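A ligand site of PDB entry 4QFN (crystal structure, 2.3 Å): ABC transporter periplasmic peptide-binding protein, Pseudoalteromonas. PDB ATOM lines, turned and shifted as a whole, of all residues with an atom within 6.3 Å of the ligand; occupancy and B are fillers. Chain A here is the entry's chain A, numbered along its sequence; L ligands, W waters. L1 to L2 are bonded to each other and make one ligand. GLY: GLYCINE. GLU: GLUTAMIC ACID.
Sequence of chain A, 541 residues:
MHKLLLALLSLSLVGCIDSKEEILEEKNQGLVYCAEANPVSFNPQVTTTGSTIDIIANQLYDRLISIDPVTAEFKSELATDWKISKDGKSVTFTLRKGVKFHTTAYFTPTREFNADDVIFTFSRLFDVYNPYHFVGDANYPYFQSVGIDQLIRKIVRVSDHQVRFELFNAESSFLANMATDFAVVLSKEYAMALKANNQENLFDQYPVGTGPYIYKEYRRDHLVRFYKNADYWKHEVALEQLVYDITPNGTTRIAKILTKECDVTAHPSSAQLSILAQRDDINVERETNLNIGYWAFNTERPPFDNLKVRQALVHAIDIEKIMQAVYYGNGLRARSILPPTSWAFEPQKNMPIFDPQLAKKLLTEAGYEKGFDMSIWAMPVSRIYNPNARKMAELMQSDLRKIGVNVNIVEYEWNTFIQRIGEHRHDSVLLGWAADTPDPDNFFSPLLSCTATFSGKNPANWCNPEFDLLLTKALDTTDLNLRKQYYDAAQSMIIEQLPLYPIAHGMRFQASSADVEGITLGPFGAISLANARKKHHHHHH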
ATOM      1  N   THR A  47      -7.286  27.781  -7.920  1.00  0.00           N
ATOM      2  CA  THR A  47      -6.870  26.990  -6.760  1.00  0.00           C
ATOM      3  C   THR A  47      -5.361  27.132  -6.498  1.00  0.00           C
ATOM      4  O   THR A  47      -4.605  27.513  -7.389  1.00  0.00           O
ATOM      5  CB  THR A  47      -7.241  25.497  -6.944  1.00  0.00           C
ATOM      6  OG1 THR A  47      -6.901  24.760  -5.770  1.00  0.00           O
ATOM      7  CG2 THR A  47      -6.514  24.895  -8.135  1.00  0.00           C
ATOM      8  N   THR A  48      -4.935  26.858  -5.265  1.00  0.00           N
ATOM      9  CA  THR A  48      -3.507  26.769  -4.982  1.00  0.00           C
ATOM     10  C   THR A  48      -3.132  25.344  -4.558  1.00  0.00           C
ATOM     11  O   THR A  48      -1.985  25.058  -4.237  1.00  0.00           O
ATOM     12  CB  THR A  48      -3.083  27.756  -3.859  1.00  0.00           C
ATOM     13  OG1 THR A  48      -3.893  27.556  -2.706  1.00  0.00           O
ATOM     14  CG2 THR A  48      -3.241  29.183  -4.300  1.00  0.00           C
ATOM     15  N   THR A  49      -4.110  24.442  -4.542  1.00  0.00           N
ATOM     16  CA  THR A  49      -3.904  23.090  -4.054  1.00  0.00           C
ATOM     17  C   THR A  49      -3.061  22.236  -5.013  1.00  0.00           C
ATOM     18  O   THR A  49      -3.454  21.984  -6.150  1.00  0.00           O
ATOM     19  CB  THR A  49      -5.258  22.398  -3.827  1.00  0.00           C
ATOM     20  OG1 THR A  49      -6.072  23.229  -3.002  1.00  0.00           O
ATOM     21  CG2 THR A  49      -5.068  21.059  -3.157  1.00  0.00           C
ATOM     22  N   GLY A  50      -1.906  21.777  -4.535  1.00  0.00           N
ATOM     23  CA  GLY A  50      -0.983  21.016  -5.360  1.00  0.00           C
ATOM     24  C   GLY A  50      -1.610  19.824  -6.056  1.00  0.00           C
ATOM     25  O   GLY A  50      -1.280  19.525  -7.199  1.00  0.00           O
ATOM     26  N   SER A  51      -2.532  19.158  -5.363  1.00  0.00           N
ATOM     27  CA  SER A  51      -3.192  17.970  -5.877  1.00  0.00           C
ATOM     28  C   SER A  51      -3.847  18.214  -7.227  1.00  0.00           C
ATOM     29  O   SER A  51      -3.810  17.367  -8.125  1.00  0.00           O
ATOM     30  CB  SER A  51      -4.277  17.538  -4.908  1.00  0.00           C
ATOM     31  OG  SER A  51      -3.775  17.596  -3.601  1.00  0.00           O
ATOM     32  N   PHE A 182       0.064  28.756 -11.865  1.00  0.00           N
ATOM     33  CA  PHE A 182      -1.255  29.371 -11.885  1.00  0.00           C
ATOM     34  C   PHE A 182      -1.424  30.299 -13.085  1.00  0.00           C
ATOM     35  O   PHE A 182      -2.541  30.582 -13.516  1.00  0.00           O
ATOM     36  CB  PHE A 182      -1.474  30.163 -10.593  1.00  0.00           C
ATOM     37  CG  PHE A 182      -1.038  29.414  -9.376  1.00  0.00           C
ATOM     38  CD1 PHE A 182      -1.696  28.272  -8.985  1.00  0.00           C
ATOM     39  CD2 PHE A 182       0.045  29.854  -8.621  1.00  0.00           C
ATOM     40  CE1 PHE A 182      -1.297  27.578  -7.864  1.00  0.00           C
ATOM     41  CE2 PHE A 182       0.440  29.167  -7.506  1.00  0.00           C
ATOM     42  CZ  PHE A 182      -0.233  28.011  -7.124  1.00  0.00           C
ATOM     43  N   MET A 379      -4.539  17.121   7.941  1.00  0.00           N
ATOM     44  CA  MET A 379      -4.660  16.665   6.563  1.00  0.00           C
ATOM     45  C   MET A 379      -4.730  15.156   6.477  1.00  0.00           C
ATOM     46  O   MET A 379      -3.972  14.447   7.141  1.00  0.00           O
ATOM     47  CB  MET A 379      -3.424  17.141   5.760  1.00  0.00           C
ATOM     48  CG  MET A 379      -2.798  18.385   6.349  1.00  0.00           C
ATOM     49  SD  MET A 379      -1.599  19.181   5.278  1.00  0.00           S
ATOM     50  CE  MET A 379      -0.104  18.500   5.968  1.00  0.00           C
ATOM     51  N   ARG A 383       1.763  15.039   2.145  1.00  0.00           N
ATOM     52  CA  ARG A 383       2.285  16.189   1.403  1.00  0.00           C
ATOM     53  C   ARG A 383       3.817  16.194   1.547  1.00  0.00           C
ATOM     54  O   ARG A 383       4.340  15.619   2.495  1.00  0.00           O
ATOM     55  CB  ARG A 383       1.733  17.524   1.948  1.00  0.00           C
ATOM     56  CG  ARG A 383       0.264  17.546   2.352  1.00  0.00           C
ATOM     57  CD  ARG A 383      -0.656  17.132   1.213  1.00  0.00           C
ATOM     58  NE  ARG A 383      -0.607  18.032   0.063  1.00  0.00           N
ATOM     59  CZ  ARG A 383      -0.577  17.625  -1.213  1.00  0.00           C
ATOM     60  NH1 ARG A 383      -0.590  16.321  -1.512  1.00  0.00           N
ATOM     61  NH2 ARG A 383      -0.540  18.533  -2.189  1.00  0.00           N
ATOM     62  N   ILE A 384       4.513  16.852   0.627  1.00  0.00           N
ATOM     63  CA  ILE A 384       5.971  16.976   0.708  1.00  0.00           C
ATOM     64  C   ILE A 384       6.404  17.469   2.070  1.00  0.00           C
ATOM     65  O   ILE A 384       7.351  16.963   2.658  1.00  0.00           O
ATOM     66  CB  ILE A 384       6.523  17.969  -0.321  1.00  0.00           C
ATOM     67  CG1 ILE A 384       6.168  17.548  -1.746  1.00  0.00           C
ATOM     68  CG2 ILE A 384       8.015  18.127  -0.149  1.00  0.00           C
ATOM     69  CD1 ILE A 384       6.448  18.620  -2.778  1.00  0.00           C
ATOM     70  N   TYR A 385       5.713  18.477   2.588  1.00  0.00           N
ATOM     71  CA  TYR A 385       6.098  19.086   3.850  1.00  0.00           C
ATOM     72  C   TYR A 385       5.559  18.383   5.114  1.00  0.00           C
ATOM     73  O   TYR A 385       5.924  18.749   6.221  1.00  0.00           O
ATOM     74  CB  TYR A 385       5.681  20.551   3.866  1.00  0.00           C
ATOM     75  CG  TYR A 385       4.242  20.748   3.500  1.00  0.00           C
ATOM     76  CD1 TYR A 385       3.236  20.528   4.444  1.00  0.00           C
ATOM     77  CD2 TYR A 385       3.883  21.135   2.212  1.00  0.00           C
ATOM     78  CE1 TYR A 385       1.912  20.701   4.112  1.00  0.00           C
ATOM     79  CE2 TYR A 385       2.553  21.298   1.871  1.00  0.00           C
ATOM     80  CZ  TYR A 385       1.568  21.078   2.835  1.00  0.00           C
ATOM     81  OH  TYR A 385       0.252  21.236   2.515  1.00  0.00           O
ATOM     82  N   TRP A 414      -9.611  15.905   1.565  1.00  0.00           N
ATOM     83  CA  TRP A 414      -8.599  16.914   1.264  1.00  0.00           C
ATOM     84  C   TRP A 414      -9.148  18.246   0.782  1.00  0.00           C
ATOM     85  O   TRP A 414      -8.848  19.295   1.354  1.00  0.00           O
ATOM     86  CB  TRP A 414      -7.592  16.348   0.267  1.00  0.00           C
ATOM     87  CG  TRP A 414      -6.457  17.247  -0.131  1.00  0.00           C
ATOM     88  CD1 TRP A 414      -5.993  17.441  -1.398  1.00  0.00           C
ATOM     89  CD2 TRP A 414      -5.605  18.014   0.734  1.00  0.00           C
ATOM     90  NE1 TRP A 414      -4.919  18.291  -1.384  1.00  0.00           N
ATOM     91  CE2 TRP A 414      -4.653  18.656  -0.093  1.00  0.00           C
ATOM     92  CE3 TRP A 414      -5.552  18.220   2.101  1.00  0.00           C
ATOM     93  CZ2 TRP A 414      -3.672  19.489   0.424  1.00  0.00           C
ATOM     94  CZ3 TRP A 414      -4.585  19.038   2.610  1.00  0.00           C
ATOM     95  CH2 TRP A 414      -3.651  19.673   1.768  1.00  0.00           C
ATOM     96  N   ILE A 418      -9.201  21.855   2.844  1.00  0.00           N
ATOM     97  CA  ILE A 418      -8.601  23.127   2.412  1.00  0.00           C
ATOM     98  C   ILE A 418      -9.625  24.263   2.423  1.00  0.00           C
ATOM     99  O   ILE A 418      -9.329  25.401   2.780  1.00  0.00           O
ATOM    100  CB  ILE A 418      -8.010  23.022   0.981  1.00  0.00           C
ATOM    101  CG1 ILE A 418      -6.760  22.139   0.953  1.00  0.00           C
ATOM    102  CG2 ILE A 418      -7.738  24.402   0.411  1.00  0.00           C
ATOM    103  CD1 ILE A 418      -5.608  22.633   1.800  1.00  0.00           C
ATOM    104  N   LEU A 431      -0.513  22.283   8.478  1.00  0.00           N
ATOM    105  CA  LEU A 431      -0.513  22.506   7.044  1.00  0.00           C
ATOM    106  C   LEU A 431       0.883  22.910   6.601  1.00  0.00           C
ATOM    107  O   LEU A 431       1.867  22.562   7.242  1.00  0.00           O
ATOM    108  CB  LEU A 431      -1.530  23.561   6.638  1.00  0.00           C
ATOM    109  CG  LEU A 431      -2.697  23.053   5.782  1.00  0.00           C
ATOM    110  CD1 LEU A 431      -3.862  24.010   5.797  1.00  0.00           C
ATOM    111  CD2 LEU A 431      -2.232  22.759   4.368  1.00  0.00           C
ATOM    112  N   GLY A 432       0.967  23.639   5.507  1.00  0.00           N
ATOM    113  CA  GLY A 432       2.248  24.051   4.991  1.00  0.00           C
ATOM    114  C   GLY A 432       2.175  24.550   3.572  1.00  0.00           C
ATOM    115  O   GLY A 432       1.086  24.829   3.067  1.00  0.00           O
ATOM    116  N   TRP A 433       3.327  24.669   2.927  1.00  0.00           N
ATOM    117  CA  TRP A 433       3.361  25.256   1.617  1.00  0.00           C
ATOM    118  C   TRP A 433       4.548  24.694   0.856  1.00  0.00           C
ATOM    119  O   TRP A 433       5.657  24.629   1.374  1.00  0.00           O
ATOM    120  CB  TRP A 433       3.459  26.772   1.746  1.00  0.00           C
ATOM    121  CG  TRP A 433       3.288  27.541   0.470  1.00  0.00           C
ATOM    122  CD1 TRP A 433       4.282  28.082  -0.304  1.00  0.00           C
ATOM    123  CD2 TRP A 433       2.054  27.886  -0.153  1.00  0.00           C
ATOM    124  NE1 TRP A 433       3.727  28.746  -1.379  1.00  0.00           N
ATOM    125  CE2 TRP A 433       2.370  28.635  -1.320  1.00  0.00           C
ATOM    126  CE3 TRP A 433       0.709  27.631   0.133  1.00  0.00           C
ATOM    127  CZ2 TRP A 433       1.387  29.125  -2.181  1.00  0.00           C
ATOM    128  CZ3 TRP A 433      -0.269  28.130  -0.720  1.00  0.00           C
ATOM    129  CH2 TRP A 433       0.073  28.872  -1.860  1.00  0.00           C
ATOM    130  N   ALA A 434       4.290  24.247  -0.370  1.00  0.00           N
ATOM    131  CA  ALA A 434       5.345  23.856  -1.282  1.00  0.00           C
ATOM    132  C   ALA A 434       5.471  24.997  -2.266  1.00  0.00           C
ATOM    133  O   ALA A 434       4.514  25.362  -2.956  1.00  0.00           O
ATOM    134  CB  ALA A 434       4.976  22.570  -2.020  1.00  0.00           C
ATOM    135  N   ALA A 435       6.660  25.582  -2.331  1.00  0.00           N
ATOM    136  CA  ALA A 435       6.845  26.823  -3.071  1.00  0.00           C
ATOM    137  C   ALA A 435       6.619  26.610  -4.561  1.00  0.00           C
ATOM    138  O   ALA A 435       6.976  25.567  -5.098  1.00  0.00           O
ATOM    139  CB  ALA A 435       8.216  27.383  -2.819  1.00  0.00           C
ATOM    140  N   ASP A 436       6.020  27.609  -5.204  1.00  0.00           N
ATOM    141  CA  ASP A 436       5.757  27.561  -6.636  1.00  0.00           C
ATOM    142  C   ASP A 436       6.924  28.183  -7.418  1.00  0.00           C
ATOM    143  O   ASP A 436       7.058  27.974  -8.616  1.00  0.00           O
ATOM    144  CB  ASP A 436       4.458  28.310  -6.950  1.00  0.00           C
ATOM    145  CG  ASP A 436       3.347  28.023  -5.920  1.00  0.00           C
ATOM    146  OD1 ASP A 436       2.788  26.901  -5.932  1.00  0.00           O
ATOM    147  OD2 ASP A 436       3.034  28.922  -5.107  1.00  0.00           O
ATOM    148  N   ASN A 442       7.096  34.113  -2.170  1.00  0.00           N
ATOM    149  CA  ASN A 442       6.138  33.047  -2.390  1.00  0.00           C
ATOM    150  C   ASN A 442       5.814  32.324  -1.083  1.00  0.00           C
ATOM    151  O   ASN A 442       4.769  31.700  -0.952  1.00  0.00           O
ATOM    152  CB  ASN A 442       6.674  32.078  -3.469  1.00  0.00           C
ATOM    153  CG  ASN A 442       5.652  31.043  -3.904  1.00  0.00           C
ATOM    154  OD1 ASN A 442       4.757  31.326  -4.719  1.00  0.00           O
ATOM    155  ND2 ASN A 442       5.783  29.825  -3.391  1.00  0.00           N
ATOM    156  N   GLY A 456      -9.392  33.758   1.694  1.00  0.00           N
ATOM    157  CA  GLY A 456      -9.572  32.354   2.018  1.00  0.00           C
ATOM    158  C   GLY A 456      -8.283  31.557   2.125  1.00  0.00           C
ATOM    159  O   GLY A 456      -8.294  30.341   1.970  1.00  0.00           O
ATOM    160  N   LYS A 457      -7.195  32.254   2.420  1.00  0.00           N
ATOM    161  CA  LYS A 457      -5.901  31.643   2.687  1.00  0.00           C
ATOM    162  C   LYS A 457      -5.399  32.135   4.038  1.00  0.00           C
ATOM    163  O   LYS A 457      -6.157  32.704   4.809  1.00  0.00           O
ATOM    164  CB  LYS A 457      -4.915  31.998   1.580  1.00  0.00           C
ATOM    165  CG  LYS A 457      -5.270  31.424   0.223  1.00  0.00           C
ATOM    166  CD  LYS A 457      -5.137  29.912   0.227  1.00  0.00           C
ATOM    167  CE  LYS A 457      -6.115  29.257  -0.727  1.00  0.00           C
ATOM    168  NZ  LYS A 457      -6.011  27.775  -0.702  1.00  0.00           N
HETATM  169  N   GLY L   1       1.890  25.516  -3.840  1.00  0.00           N
HETATM  170  CA  GLY L   1       0.748  25.609  -2.952  1.00  0.00           C
HETATM  171  C   GLY L   1       0.691  24.502  -1.901  1.00  0.00           C
HETATM  172  O   GLY L   1       1.717  23.953  -1.504  1.00  0.00           O
HETATM  173  N   GLU L   2      -0.526  24.186  -1.445  1.00  0.00           N
HETATM  174  CA  GLU L   2      -0.709  23.223  -0.356  1.00  0.00           C
HETATM  175  C   GLU L   2      -0.502  21.781  -0.796  1.00  0.00           C
HETATM  176  O   GLU L   2      -0.698  21.422  -1.953  1.00  0.00           O
HETATM  177  CB  GLU L   2      -2.088  23.394   0.297  1.00  0.00           C
HETATM  178  CG  GLU L   2      -2.320  24.767   0.892  1.00  0.00           C
HETATM  179  CD  GLU L   2      -3.071  25.714  -0.047  1.00  0.00           C
HETATM  180  OE1 GLU L   2      -3.555  26.764   0.425  1.00  0.00           O
HETATM  181  OE2 GLU L   2      -3.184  25.394  -1.259  1.00  0.00           O
HETATM  182  OXT GLU L   2      -0.144  20.935   0.021  1.00  0.00           O
HETATM  183  O   HOH W   1      -2.723  27.828   2.698  1.00  0.00           O
HETATM  184  O   HOH W   2       1.850  21.115  -2.319  1.00  0.00           O
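The side-chain amide nitrogen (ND2) of Asn 442 lies close to the backbone NH (N) of Asp 436, 2.9 Å away. The side-chain amino group (NZ) of Lys 457 lies within hydrogen-bond range of the side-chain hydroxyl (OG1) of Thr 48 (2.9 Å). The indole nitrogen of Trp 433 sits close to the side-chain amide nitrogen of Asn 442, 3.1 Å away. The backbone NH of Thr 49 is in hydrogen-bond range of the side-chain hydroxyl of Thr 47. NE1 of Trp 414 sits at hydrogen-bond distance from OG of Ser 51, 2.6 Å away.
The side-chain hydroxyl of Tyr 385 is in hydrogen-bond range of an oxygen (OXT) of GLU L2 (2.5 Å). OD1 of Asp 436 is in salt-bridge range of N of GLY L1, 2.7 Å away. A nitrogen (N) of GLU L2 lies close to the backbone carbonyl oxygen of Thr 48 (3.3 Å). OG1 of Thr 48 lies within hydrogen-bond range of OE2 of GLU L2 (2.7 Å). N of Ala 434 is in hydrogen-bond range of O of GLY L1. The backbone carbonyl oxygen (O) of Ala 434 sits at hydrogen-bond distance from a nitrogen (N) of GLY L1 (2.8 Å). The backbone NH (N) of Gly 50 sits at hydrogen-bond distance from an oxygen (O) of GLU L2 (2.9 Å). NZ of Lys 457 is in salt-bridge range of OE1 of GLU L2, 2.9 Å away. The guanidinium group of Arg 383 lies within salt-bridge range of an oxygen (O) of GLU L2 (2.9 Å).
Merely in contact with the ligand: Trp 433 (3.5 Å), Thr 49 (3.5 Å), Trp 414 (3.8 Å) and Ile 418 (3.9 Å). Hydrophobic or aromatic side chains that line the ligand: Tyr 385, Trp 414, Ile 418, Trp 433 and Ala 434.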
